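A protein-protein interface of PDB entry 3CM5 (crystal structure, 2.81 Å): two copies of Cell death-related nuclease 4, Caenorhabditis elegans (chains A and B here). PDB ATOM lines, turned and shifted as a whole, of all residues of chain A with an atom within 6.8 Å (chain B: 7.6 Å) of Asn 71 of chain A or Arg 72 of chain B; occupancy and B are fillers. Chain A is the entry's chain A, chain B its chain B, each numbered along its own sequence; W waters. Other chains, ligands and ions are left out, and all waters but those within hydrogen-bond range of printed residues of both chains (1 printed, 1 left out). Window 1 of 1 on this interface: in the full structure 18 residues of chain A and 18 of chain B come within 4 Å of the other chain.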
ATOM      1  N   THR A  29      23.271 -21.234   6.824  1.00  0.00           N
ATOM      2  CA  THR A  29      23.686 -19.826   6.953  1.00  0.00           C
ATOM      3  C   THR A  29      22.488 -18.909   6.736  1.00  0.00           C
ATOM      4  O   THR A  29      21.521 -19.264   6.050  1.00  0.00           O
ATOM      5  CB  THR A  29      24.829 -19.413   5.956  1.00  0.00           C
ATOM      6  OG1 THR A  29      24.362 -19.420   4.603  1.00  0.00           O
ATOM      7  CG2 THR A  29      26.031 -20.330   6.066  1.00  0.00           C
ATOM      8  N   TYR A  37      19.386 -13.807   0.560  1.00  0.00           N
ATOM      9  CA  TYR A  37      20.527 -14.457   1.131  1.00  0.00           C
ATOM     10  C   TYR A  37      20.754 -15.868   0.575  1.00  0.00           C
ATOM     11  O   TYR A  37      19.859 -16.709   0.641  1.00  0.00           O
ATOM     12  CB  TYR A  37      20.383 -14.485   2.657  1.00  0.00           C
ATOM     13  CG  TYR A  37      21.700 -14.785   3.339  1.00  0.00           C
ATOM     14  CD1 TYR A  37      22.570 -13.745   3.736  1.00  0.00           C
ATOM     15  CD2 TYR A  37      22.109 -16.103   3.553  1.00  0.00           C
ATOM     16  CE1 TYR A  37      23.784 -14.019   4.348  1.00  0.00           C
ATOM     17  CE2 TYR A  37      23.325 -16.377   4.169  1.00  0.00           C
ATOM     18  CZ  TYR A  37      24.151 -15.335   4.557  1.00  0.00           C
ATOM     19  OH  TYR A  37      25.339 -15.638   5.155  1.00  0.00           O
ATOM     20  N   PRO A  38      21.966 -16.142   0.063  1.00  0.00           N
ATOM     21  CA  PRO A  38      22.294 -17.400  -0.587  1.00  0.00           C
ATOM     22  C   PRO A  38      22.564 -18.537   0.414  1.00  0.00           C
ATOM     23  O   PRO A  38      23.715 -19.010   0.538  1.00  0.00           O
ATOM     24  CB  PRO A  38      23.575 -17.059  -1.341  1.00  0.00           C
ATOM     25  CG  PRO A  38      24.225 -16.065  -0.523  1.00  0.00           C
ATOM     26  CD  PRO A  38      23.131 -15.247   0.104  1.00  0.00           C
ATOM     27  N   CYS A  39      21.512 -18.981   1.104  1.00  0.00           N
ATOM     28  CA  CYS A  39      21.640 -19.981   2.169  1.00  0.00           C
ATOM     29  C   CYS A  39      22.516 -21.121   1.805  1.00  0.00           C
ATOM     30  O   CYS A  39      22.360 -21.704   0.743  1.00  0.00           O
ATOM     31  CB  CYS A  39      20.289 -20.549   2.528  1.00  0.00           C
ATOM     32  SG  CYS A  39      19.352 -19.309   3.362  1.00  0.00           S
ATOM     33  N   GLU A  40      23.444 -21.442   2.690  1.00  0.00           N
ATOM     34  CA  GLU A  40      24.201 -22.667   2.542  1.00  0.00           C
ATOM     35  C   GLU A  40      23.948 -23.557   3.754  1.00  0.00           C
ATOM     36  O   GLU A  40      23.793 -23.059   4.874  1.00  0.00           O
ATOM     37  CB  GLU A  40      25.675 -22.370   2.390  1.00  0.00           C
ATOM     38  CG  GLU A  40      26.096 -21.997   0.996  1.00  0.00           C
ATOM     39  CD  GLU A  40      27.472 -21.360   1.004  1.00  0.00           C
ATOM     40  OE1 GLU A  40      27.626 -20.311   1.679  1.00  0.00           O
ATOM     41  OE2 GLU A  40      28.396 -21.915   0.360  1.00  0.00           O
ATOM     42  N   ILE A  42      24.622 -25.746   6.817  1.00  0.00           N
ATOM     43  CA  ILE A  42      25.697 -25.835   7.815  1.00  0.00           C
ATOM     44  C   ILE A  42      25.580 -27.048   8.753  1.00  0.00           C
ATOM     45  O   ILE A  42      26.547 -27.442   9.400  1.00  0.00           O
ATOM     46  CB  ILE A  42      25.906 -24.514   8.594  1.00  0.00           C
ATOM     47  CG1 ILE A  42      24.630 -24.029   9.266  1.00  0.00           C
ATOM     48  CG2 ILE A  42      26.438 -23.464   7.667  1.00  0.00           C
ATOM     49  CD1 ILE A  42      24.879 -22.921  10.296  1.00  0.00           C
ATOM     50  N   PRO A  68      30.374 -23.811   4.678  1.00  0.00           N
ATOM     51  CA  PRO A  68      29.916 -23.037   3.506  1.00  0.00           C
ATOM     52  C   PRO A  68      31.077 -22.512   2.677  1.00  0.00           C
ATOM     53  O   PRO A  68      32.198 -22.394   3.189  1.00  0.00           O
ATOM     54  CB  PRO A  68      29.198 -21.851   4.129  1.00  0.00           C
ATOM     55  CG  PRO A  68      29.761 -21.736   5.499  1.00  0.00           C
ATOM     56  CD  PRO A  68      30.083 -23.119   5.943  1.00  0.00           C
ATOM     57  N   VAL A  69      30.836 -22.202   1.407  1.00  0.00           N
ATOM     58  CA  VAL A  69      31.897 -21.569   0.613  1.00  0.00           C
ATOM     59  C   VAL A  69      31.622 -20.095   0.310  1.00  0.00           C
ATOM     60  O   VAL A  69      32.541 -19.276   0.365  1.00  0.00           O
ATOM     61  CB  VAL A  69      32.279 -22.376  -0.646  1.00  0.00           C
ATOM     62  CG1 VAL A  69      32.779 -23.724  -0.217  1.00  0.00           C
ATOM     63  CG2 VAL A  69      31.098 -22.531  -1.598  1.00  0.00           C
ATOM     64  N   LEU A  70      30.361 -19.763   0.041  1.00  0.00           N
ATOM     65  CA  LEU A  70      29.972 -18.389  -0.229  1.00  0.00           C
ATOM     66  C   LEU A  70      30.053 -17.458   0.978  1.00  0.00           C
ATOM     67  O   LEU A  70      30.491 -16.316   0.862  1.00  0.00           O
ATOM     68  CB  LEU A  70      28.570 -18.343  -0.815  1.00  0.00           C
ATOM     69  CG  LEU A  70      28.307 -19.101  -2.115  1.00  0.00           C
ATOM     70  CD1 LEU A  70      26.867 -18.814  -2.496  1.00  0.00           C
ATOM     71  CD2 LEU A  70      29.265 -18.758  -3.261  1.00  0.00           C
ATOM     72  N   ASN A  71      29.615 -17.925   2.130  1.00  0.00           N
ATOM     73  CA  ASN A  71      29.680 -17.103   3.308  1.00  0.00           C
ATOM     74  C   ASN A  71      30.317 -17.848   4.466  1.00  0.00           C
ATOM     75  O   ASN A  71      29.619 -18.340   5.374  1.00  0.00           O
ATOM     76  CB  ASN A  71      28.288 -16.583   3.680  1.00  0.00           C
ATOM     77  CG  ASN A  71      27.823 -15.441   2.779  1.00  0.00           C
ATOM     78  OD1 ASN A  71      26.841 -15.578   2.029  1.00  0.00           O
ATOM     79  ND2 ASN A  71      28.511 -14.298   2.866  1.00  0.00           N
ATOM     80  N   ARG A  72      31.646 -17.886   4.457  1.00  0.00           N
ATOM     81  CA  ARG A  72      32.382 -18.743   5.372  1.00  0.00           C
ATOM     82  C   ARG A  72      32.244 -18.424   6.857  1.00  0.00           C
ATOM     83  O   ARG A  72      32.400 -19.303   7.692  1.00  0.00           O
ATOM     84  CB  ARG A  72      33.832 -18.845   4.942  1.00  0.00           C
ATOM     85  CG  ARG A  72      33.927 -19.391   3.515  1.00  0.00           C
ATOM     86  CD  ARG A  72      35.334 -19.842   3.126  1.00  0.00           C
ATOM     87  NE  ARG A  72      35.952 -20.703   4.140  1.00  0.00           N
ATOM     88  CZ  ARG A  72      37.238 -21.068   4.146  1.00  0.00           C
ATOM     89  NH1 ARG A  72      38.082 -20.664   3.181  1.00  0.00           N
ATOM     90  NH2 ARG A  72      37.676 -21.851   5.131  1.00  0.00           N
ATOM     91  N   THR A  73      31.935 -17.174   7.184  1.00  0.00           N
ATOM     92  CA  THR A  73      31.835 -16.736   8.573  1.00  0.00           C
ATOM     93  C   THR A  73      30.393 -16.597   8.921  1.00  0.00           C
ATOM     94  O   THR A  73      29.683 -15.851   8.269  1.00  0.00           O
ATOM     95  CB  THR A  73      32.465 -15.358   8.757  1.00  0.00           C
ATOM     96  OG1 THR A  73      33.843 -15.437   8.427  1.00  0.00           O
ATOM     97  CG2 THR A  73      32.334 -14.888  10.187  1.00  0.00           C
ATOM     98  N   LEU A  74      29.948 -17.277   9.959  1.00  0.00           N
ATOM     99  CA  LEU A  74      28.544 -17.244  10.287  1.00  0.00           C
ATOM    100  C   LEU A  74      28.251 -15.951  10.977  1.00  0.00           C
ATOM    101  O   LEU A  74      28.899 -15.640  11.951  1.00  0.00           O
ATOM    102  CB  LEU A  74      28.197 -18.382  11.237  1.00  0.00           C
ATOM    103  CG  LEU A  74      28.329 -19.853  10.862  1.00  0.00           C
ATOM    104  CD1 LEU A  74      27.542 -20.634  11.908  1.00  0.00           C
ATOM    105  CD2 LEU A  74      27.798 -20.126   9.473  1.00  0.00           C
ATOM    106  N   THR A  75      27.274 -15.201  10.491  1.00  0.00           N
ATOM    107  CA  THR A  75      26.836 -13.980  11.169  1.00  0.00           C
ATOM    108  C   THR A  75      26.484 -14.276  12.622  1.00  0.00           C
ATOM    109  O   THR A  75      26.064 -15.382  12.934  1.00  0.00           O
ATOM    110  CB  THR A  75      25.594 -13.401  10.502  1.00  0.00           C
ATOM    111  OG1 THR A  75      24.460 -14.215  10.830  1.00  0.00           O
ATOM    112  CG2 THR A  75      25.769 -13.371   9.007  1.00  0.00           C
ATOM    113  N   GLN A  86      31.275 -21.159  15.390  1.00  0.00           N
ATOM    114  CA  GLN A  86      32.096 -21.023  14.188  1.00  0.00           C
ATOM    115  C   GLN A  86      33.171 -22.106  14.045  1.00  0.00           C
ATOM    116  O   GLN A  86      33.475 -22.536  12.926  1.00  0.00           O
ATOM    117  CB  GLN A  86      32.687 -19.614  14.121  1.00  0.00           C
ATOM    118  CG  GLN A  86      33.552 -19.330  12.911  1.00  0.00           C
ATOM    119  CD  GLN A  86      32.788 -19.323  11.584  1.00  0.00           C
ATOM    120  OE1 GLN A  86      31.788 -18.627  11.424  1.00  0.00           O
ATOM    121  NE2 GLN A  86      33.290 -20.076  10.616  1.00  0.00           N
ATOM    122  N   ILE A  89      31.999 -25.109  12.172  1.00  0.00           N
ATOM    123  CA  ILE A  89      31.922 -25.066  10.713  1.00  0.00           C
ATOM    124  C   ILE A  89      33.299 -25.002  10.025  1.00  0.00           C
ATOM    125  O   ILE A  89      33.472 -25.591   8.953  1.00  0.00           O
ATOM    126  CB  ILE A  89      30.847 -24.065  10.145  1.00  0.00           C
ATOM    127  CG1 ILE A  89      31.317 -22.638  10.210  1.00  0.00           C
ATOM    128  CG2 ILE A  89      29.486 -24.232  10.814  1.00  0.00           C
ATOM    129  CD1 ILE A  89      31.779 -22.179   8.848  1.00  0.00           C
ATOM    130  N   HIS A 300      20.151 -10.966  -5.520  1.00  0.00           N
ATOM    131  CA  HIS A 300      21.498 -11.428  -5.246  1.00  0.00           C
ATOM    132  C   HIS A 300      21.611 -12.936  -5.292  1.00  0.00           C
ATOM    133  O   HIS A 300      22.468 -13.466  -5.987  1.00  0.00           O
ATOM    134  CB  HIS A 300      22.013 -10.894  -3.914  1.00  0.00           C
ATOM    135  CG  HIS A 300      23.309 -11.513  -3.479  1.00  0.00           C
ATOM    136  ND1 HIS A 300      24.480 -11.373  -4.193  1.00  0.00           N
ATOM    137  CD2 HIS A 300      23.613 -12.282  -2.406  1.00  0.00           C
ATOM    138  CE1 HIS A 300      25.449 -12.031  -3.582  1.00  0.00           C
ATOM    139  NE2 HIS A 300      24.949 -12.588  -2.495  1.00  0.00           N
ATOM    140  N   ILE A 304      24.480 -15.077  -7.606  1.00  0.00           N
ATOM    141  CA  ILE A 304      25.592 -15.945  -7.156  1.00  0.00           C
ATOM    142  C   ILE A 304      25.317 -17.398  -7.444  1.00  0.00           C
ATOM    143  O   ILE A 304      26.243 -18.147  -7.662  1.00  0.00           O
ATOM    144  CB  ILE A 304      25.989 -15.843  -5.658  1.00  0.00           C
ATOM    145  CG1 ILE A 304      24.939 -15.120  -4.867  1.00  0.00           C
ATOM    146  CG2 ILE A 304      27.357 -15.217  -5.449  1.00  0.00           C
ATOM    147  CD1 ILE A 304      23.952 -16.054  -4.344  1.00  0.00           C
ATOM    148  N   THR B  29      33.899  -5.688   4.527  1.00  0.00           N
ATOM    149  CA  THR B  29      32.863  -6.561   5.070  1.00  0.00           C
ATOM    150  C   THR B  29      32.980  -6.517   6.592  1.00  0.00           C
ATOM    151  O   THR B  29      34.051  -6.205   7.141  1.00  0.00           O
ATOM    152  CB  THR B  29      32.970  -8.032   4.561  1.00  0.00           C
ATOM    153  OG1 THR B  29      34.197  -8.637   4.999  1.00  0.00           O
ATOM    154  CG2 THR B  29      32.912  -8.095   3.038  1.00  0.00           C
ATOM    155  N   TYR B  37      36.111 -11.570  12.894  1.00  0.00           N
ATOM    156  CA  TYR B  37      35.555 -11.539  11.556  1.00  0.00           C
ATOM    157  C   TYR B  37      36.636 -11.185  10.525  1.00  0.00           C
ATOM    158  O   TYR B  37      37.314 -10.169  10.676  1.00  0.00           O
ATOM    159  CB  TYR B  37      34.443 -10.501  11.521  1.00  0.00           C
ATOM    160  CG  TYR B  37      33.607 -10.544  10.272  1.00  0.00           C
ATOM    161  CD1 TYR B  37      32.422 -11.263  10.241  1.00  0.00           C
ATOM    162  CD2 TYR B  37      33.997  -9.861   9.117  1.00  0.00           C
ATOM    163  CE1 TYR B  37      31.646 -11.309   9.101  1.00  0.00           C
ATOM    164  CE2 TYR B  37      33.223  -9.902   7.968  1.00  0.00           C
ATOM    165  CZ  TYR B  37      32.045 -10.627   7.969  1.00  0.00           C
ATOM    166  OH  TYR B  37      31.249 -10.676   6.848  1.00  0.00           O
ATOM    167  N   GLU B  40      37.208  -8.183   4.719  1.00  0.00           N
ATOM    168  CA  GLU B  40      37.715  -8.039   3.377  1.00  0.00           C
ATOM    169  C   GLU B  40      37.330  -6.664   2.856  1.00  0.00           C
ATOM    170  O   GLU B  40      36.247  -6.150   3.145  1.00  0.00           O
ATOM    171  CB  GLU B  40      37.156  -9.119   2.469  1.00  0.00           C
ATOM    172  CG  GLU B  40      37.407 -10.539   2.925  1.00  0.00           C
ATOM    173  CD  GLU B  40      36.740 -11.555   2.012  1.00  0.00           C
ATOM    174  OE1 GLU B  40      35.617 -11.994   2.329  1.00  0.00           O
ATOM    175  OE2 GLU B  40      37.328 -11.905   0.969  1.00  0.00           O
ATOM    176  N   ILE B  42      35.855  -3.951   0.638  1.00  0.00           N
ATOM    177  CA  ILE B  42      34.792  -3.810  -0.348  1.00  0.00           C
ATOM    178  C   ILE B  42      34.752  -2.468  -1.084  1.00  0.00           C
ATOM    179  O   ILE B  42      34.105  -2.341  -2.121  1.00  0.00           O
ATOM    180  CB  ILE B  42      33.439  -4.119   0.247  1.00  0.00           C
ATOM    181  CG1 ILE B  42      33.201  -3.263   1.482  1.00  0.00           C
ATOM    182  CG2 ILE B  42      33.380  -5.589   0.576  1.00  0.00           C
ATOM    183  CD1 ILE B  42      31.782  -3.274   1.974  1.00  0.00           C
ATOM    184  N   LYS B  67      35.024  -7.010  -4.710  1.00  0.00           N
ATOM    185  CA  LYS B  67      34.265  -8.237  -4.443  1.00  0.00           C
ATOM    186  C   LYS B  67      35.049  -9.160  -3.521  1.00  0.00           C
ATOM    187  O   LYS B  67      36.134  -9.641  -3.864  1.00  0.00           O
ATOM    188  CB  LYS B  67      33.919  -8.948  -5.752  1.00  0.00           C
ATOM    189  CG  LYS B  67      32.958 -10.118  -5.595  1.00  0.00           C
ATOM    190  CD  LYS B  67      32.540 -10.695  -6.957  1.00  0.00           C
ATOM    191  CE  LYS B  67      33.535 -11.740  -7.444  1.00  0.00           C
ATOM    192  NZ  LYS B  67      33.377 -12.073  -8.884  1.00  0.00           N
ATOM    193  N   PRO B  68      34.520  -9.382  -2.323  1.00  0.00           N
ATOM    194  CA  PRO B  68      35.126 -10.314  -1.366  1.00  0.00           C
ATOM    195  C   PRO B  68      34.923 -11.777  -1.764  1.00  0.00           C
ATOM    196  O   PRO B  68      34.006 -12.089  -2.527  1.00  0.00           O
ATOM    197  CB  PRO B  68      34.394 -10.006  -0.058  1.00  0.00           C
ATOM    198  CG  PRO B  68      33.110  -9.379  -0.460  1.00  0.00           C
ATOM    199  CD  PRO B  68      33.320  -8.722  -1.796  1.00  0.00           C
ATOM    200  N   VAL B  69      35.779 -12.665  -1.268  1.00  0.00           N
ATOM    201  CA  VAL B  69      35.605 -14.084  -1.564  1.00  0.00           C
ATOM    202  C   VAL B  69      35.255 -14.965  -0.363  1.00  0.00           C
ATOM    203  O   VAL B  69      34.662 -16.028  -0.567  1.00  0.00           O
ATOM    204  CB  VAL B  69      36.772 -14.685  -2.377  1.00  0.00           C
ATOM    205  CG1 VAL B  69      37.137 -13.757  -3.506  1.00  0.00           C
ATOM    206  CG2 VAL B  69      37.988 -14.937  -1.495  1.00  0.00           C
ATOM    207  N   LEU B  70      35.600 -14.550   0.859  1.00  0.00           N
ATOM    208  CA  LEU B  70      35.294 -15.364   2.038  1.00  0.00           C
ATOM    209  C   LEU B  70      33.865 -15.175   2.487  1.00  0.00           C
ATOM    210  O   LEU B  70      33.177 -16.141   2.818  1.00  0.00           O
ATOM    211  CB  LEU B  70      36.208 -15.032   3.194  1.00  0.00           C
ATOM    212  CG  LEU B  70      37.591 -15.673   3.296  1.00  0.00           C
ATOM    213  CD1 LEU B  70      38.356 -15.658   1.994  1.00  0.00           C
ATOM    214  CD2 LEU B  70      38.386 -14.926   4.360  1.00  0.00           C
ATOM    215  N   ASN B  71      33.424 -13.921   2.526  1.00  0.00           N
ATOM    216  CA  ASN B  71      32.046 -13.600   2.871  1.00  0.00           C
ATOM    217  C   ASN B  71      31.424 -12.740   1.801  1.00  0.00           C
ATOM    218  O   ASN B  71      31.505 -11.507   1.842  1.00  0.00           O
ATOM    219  CB  ASN B  71      31.967 -12.946   4.240  1.00  0.00           C
ATOM    220  CG  ASN B  71      32.310 -13.912   5.348  1.00  0.00           C
ATOM    221  OD1 ASN B  71      33.213 -13.658   6.148  1.00  0.00           O
ATOM    222  ND2 ASN B  71      31.609 -15.044   5.391  1.00  0.00           N
ATOM    223  N   ARG B  72      30.789 -13.419   0.851  1.00  0.00           N
ATOM    224  CA  ARG B  72      30.349 -12.812  -0.398  1.00  0.00           C
ATOM    225  C   ARG B  72      29.083 -11.980  -0.303  1.00  0.00           C
ATOM    226  O   ARG B  72      28.856 -11.127  -1.143  1.00  0.00           O
ATOM    227  CB  ARG B  72      30.202 -13.890  -1.468  1.00  0.00           C
ATOM    228  CG  ARG B  72      31.299 -13.857  -2.479  1.00  0.00           C
ATOM    229  CD  ARG B  72      31.452 -15.176  -3.157  1.00  0.00           C
ATOM    230  NE  ARG B  72      32.325 -16.080  -2.406  1.00  0.00           N
ATOM    231  CZ  ARG B  72      32.917 -17.162  -2.934  1.00  0.00           C
ATOM    232  NH1 ARG B  72      32.723 -17.474  -4.223  1.00  0.00           N
ATOM    233  NH2 ARG B  72      33.705 -17.934  -2.175  1.00  0.00           N
ATOM    234  N   THR B  73      28.264 -12.233   0.712  1.00  0.00           N
ATOM    235  CA  THR B  73      27.014 -11.515   0.898  1.00  0.00           C
ATOM    236  C   THR B  73      27.157 -10.570   2.072  1.00  0.00           C
ATOM    237  O   THR B  73      27.307 -11.000   3.205  1.00  0.00           O
ATOM    238  CB  THR B  73      25.856 -12.466   1.182  1.00  0.00           C
ATOM    239  OG1 THR B  73      25.740 -13.369   0.092  1.00  0.00           O
ATOM    240  CG2 THR B  73      24.544 -11.700   1.352  1.00  0.00           C
ATOM    241  N   LEU B  74      27.086  -9.277   1.780  1.00  0.00           N
ATOM    242  CA  LEU B  74      27.192  -8.259   2.798  1.00  0.00           C
ATOM    243  C   LEU B  74      26.160  -8.480   3.861  1.00  0.00           C
ATOM    244  O   LEU B  74      25.038  -8.885   3.595  1.00  0.00           O
ATOM    245  CB  LEU B  74      27.026  -6.870   2.191  1.00  0.00           C
ATOM    246  CG  LEU B  74      28.283  -6.105   1.778  1.00  0.00           C
ATOM    247  CD1 LEU B  74      29.381  -7.001   1.214  1.00  0.00           C
ATOM    248  CD2 LEU B  74      27.898  -5.028   0.775  1.00  0.00           C
ATOM    249  N   THR B  75      26.573  -8.231   5.084  1.00  0.00           N
ATOM    250  CA  THR B  75      25.708  -8.306   6.225  1.00  0.00           C
ATOM    251  C   THR B  75      24.730  -7.150   6.135  1.00  0.00           C
ATOM    252  O   THR B  75      25.072  -6.098   5.609  1.00  0.00           O
ATOM    253  CB  THR B  75      26.606  -8.197   7.430  1.00  0.00           C
ATOM    254  OG1 THR B  75      26.777  -9.499   7.986  1.00  0.00           O
ATOM    255  CG2 THR B  75      26.071  -7.292   8.444  1.00  0.00           C
ATOM    256  N   GLN B  86      24.378  -4.424  -2.213  1.00  0.00           N
ATOM    257  CA  GLN B  86      24.948  -5.710  -2.601  1.00  0.00           C
ATOM    258  C   GLN B  86      25.308  -5.739  -4.095  1.00  0.00           C
ATOM    259  O   GLN B  86      26.318  -6.329  -4.483  1.00  0.00           O
ATOM    260  CB  GLN B  86      24.016  -6.863  -2.192  1.00  0.00           C
ATOM    261  CG  GLN B  86      24.485  -8.270  -2.588  1.00  0.00           C
ATOM    262  CD  GLN B  86      25.801  -8.713  -1.929  1.00  0.00           C
ATOM    263  OE1 GLN B  86      26.018  -8.535  -0.724  1.00  0.00           O
ATOM    264  NE2 GLN B  86      26.671  -9.318  -2.725  1.00  0.00           N
ATOM    265  N   ILE B  89      28.884  -4.601  -5.189  1.00  0.00           N
ATOM    266  CA  ILE B  89      29.940  -5.575  -4.984  1.00  0.00           C
ATOM    267  C   ILE B  89      29.858  -6.848  -5.883  1.00  0.00           C
ATOM    268  O   ILE B  89      30.882  -7.486  -6.164  1.00  0.00           O
ATOM    269  CB  ILE B  89      30.142  -5.929  -3.493  1.00  0.00           C
ATOM    270  CG1 ILE B  89      29.092  -6.896  -3.030  1.00  0.00           C
ATOM    271  CG2 ILE B  89      30.131  -4.706  -2.604  1.00  0.00           C
ATOM    272  CD1 ILE B  89      29.741  -8.081  -2.383  1.00  0.00           C
ATOM    273  N   ASP B  90      28.661  -7.204  -6.352  1.00  0.00           N
ATOM    274  CA  ASP B  90      28.507  -8.418  -7.192  1.00  0.00           C
ATOM    275  C   ASP B  90      29.071  -8.212  -8.594  1.00  0.00           C
ATOM    276  O   ASP B  90      29.416  -9.188  -9.293  1.00  0.00           O
ATOM    277  CB  ASP B  90      27.048  -8.900  -7.282  1.00  0.00           C
ATOM    278  CG  ASP B  90      26.603  -9.676  -6.051  1.00  0.00           C
ATOM    279  OD1 ASP B  90      25.389  -9.929  -5.925  1.00  0.00           O
ATOM    280  OD2 ASP B  90      27.459 -10.024  -5.204  1.00  0.00           O
ATOM    281  N   ILE B 304      41.232 -18.693   9.312  1.00  0.00           N
ATOM    282  CA  ILE B 304      40.854 -18.581   7.905  1.00  0.00           C
ATOM    283  C   ILE B 304      41.939 -17.977   7.010  1.00  0.00           C
ATOM    284  O   ILE B 304      42.049 -18.342   5.856  1.00  0.00           O
ATOM    285  CB  ILE B 304      39.519 -17.855   7.710  1.00  0.00           C
ATOM    286  CG1 ILE B 304      38.882 -18.321   6.398  1.00  0.00           C
ATOM    287  CG2 ILE B 304      39.707 -16.346   7.778  1.00  0.00           C
ATOM    288  CD1 ILE B 304      37.389 -18.123   6.329  1.00  0.00           C
HETATM  289  O   HOH W   1      27.347 -13.650   5.266  1.00  0.00           O
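Water W1 lies within hydrogen-bond range of ND2 of Asn 71 of chain A, OH of Tyr 37 of chain A and O of Thr 73 of chain B.
The side-chain carboxylate (OE2) of Glu 40 of chain A sits at hydrogen-bond distance from the backbone NH (N) of Val 69 of chain A, at 2.7 Å.
O of Arg 72 of chain B is in hydrogen-bond range of NE2 of Gln 86 of chain B, 3.2 Å away.
The side-chain hydroxyl of Tyr 37 of chain A sits close to the side-chain amide oxygen of Asn 71 of chain A.
The side-chain sulfur (SG) of Cys 39 of chain A sits at hydrogen-bond distance from the backbone carbonyl oxygen (O) of Tyr 37 of chain A, 3.8 Å away.
The backbone NH (N) of Leu 70 of chain B sits at hydrogen-bond distance from the side-chain carboxylate (OE1) of Glu 40 of chain B, 2.9 Å away.
The backbone NH (N) of Leu 74 of chain B sits at hydrogen-bond distance from the side-chain amide oxygen (OE1) of Gln 86 of chain B (2.8 Å).
Tyr 37 of chain A touches Thr 73 of chain B, and with the chains exchanged Thr 73 of chain A touches Tyr 37 of chain B.
Leu 70 of chain A touches Asn 71 of chain B, and with the chains exchanged Asn 71 of chain A touches Leu 70 of chain B.
Leu 70 of chain A touches Arg 72 of chain B, and with the chains exchanged Arg 72 of chain A touches Leu 70 of chain B.
Asn 71 of chain A touches Thr 73 of chain B, and with the chains exchanged Thr 73 of chain A touches Asn 71 of chain B.
Hydrophobic or aromatic side chains of chain A within 4 Å of the printed part of chain B: Tyr 37, Pro 38, Leu 70 and His 300.
Hydrophobic or aromatic side chains of chain B within 4 Å of the printed part of chain A: Tyr 37 and Ile 304.
Among the printed residues, 19 pairs touch across the chains.
Among the printed residues, no Asp or Glu carboxylate lies within 4 Å of a Lys or Arg side-chain nitrogen of the other chain.
Of the printed residues of chain B, Leu 70 of chain A touches Leu 70 (3.3 Å), Asn 71 (3.7 Å) and Arg 72 (2.9 Å).
Asn 71 of chain A touches four residues of chain B.
Printed residues of chain B within 4 Å of His 300 of chain A: Thr 73, Gln 86 and Asp 90.
Glu 40 of chain B touches none of the printed residues of chain A.
Printed residues of chain A within 4 Å of Val 69 of chain B: Val 69 (3.99 Å).
Printed residues of chain A within 4 Å of Asn 71 of chain B: Leu 70 (3.7 Å), Asn 71 (3.2 Å), Arg 72 (3.0 Å) and Thr 73 (2.8 Å).
Of chain A, only Val 69, Leu 70 and Asn 71 come within 4 Å of Arg 72 of chain B.
Printed residues of chain A within 4 Å of Thr 73 of chain B: Tyr 37 (3.7 Å), Pro 38 (3.2 Å), Asn 71 (3.0 Å) and His 300 (2.8 Å).
Thr 75 of chain B touches none of the printed residues of chain A.
The nearest printed residue of chain A that does not touch Gln 86 of chain B is Ile 304 of chain A (6.4 Å).
Among the printed residues, pairs that only touch across the chains: Tyr 37 of chain A with Thr 73 of chain B, Pro 38 of chain A with Thr 73 of chain B, Val 69 of chain A with Val 69 of chain B, Leu 70 of chain A with Asn 71 of chain B, Asn 71 of chain A with Leu 70 of chain B, Asn 71 of chain A with Asn 71 of chain B, Arg 72 of chain A with Ile 304 of chain B and Thr 73 of chain A with Tyr 37 of chain B.
The backbone NH (N) of Arg 72 of chain A lies close to the side-chain amide nitrogen (ND2) of Asn 71 of chain B.
OG1 of Thr 73 of chain B sits at hydrogen-bond distance from NE2 of His 300 of chain A (2.8 Å).
The backbone NH (N) of Arg 72 of chain A is in hydrogen-bond range of the backbone carbonyl oxygen (O) of Leu 70 of chain B (2.8 Å).
The backbone carbonyl oxygen (O) of Val 69 of chain A sits at hydrogen-bond distance from the guanidinium group (NH2) of Arg 72 of chain B, 3.1 Å away.
N of Arg 72 of chain B lies within hydrogen-bond range of O of Leu 70 of chain A (2.9 Å).
ND2 of Asn 71 of chain A lies close to N of Arg 72 of chain B.
The backbone carbonyl oxygen (O) of Leu 70 of chain A sits close to the backbone carbonyl oxygen (O) of Leu 70 of chain B, at 3.3 Å.
ND1 of His 300 of chain A lies within hydrogen-bond range of OD1 of Asp 90 of chain B (2.4 Å).
NE2 of Gln 86 of chain B sits close to ND1 of His 300 of chain A, 3.3 Å away.
ND2 of Asn 71 of chain A lies close to N of Thr 73 of chain B (3.0 Å).
ND2 of Asn 71 of chain B sits close to N of Thr 73 of chain A, at 2.8 Å.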
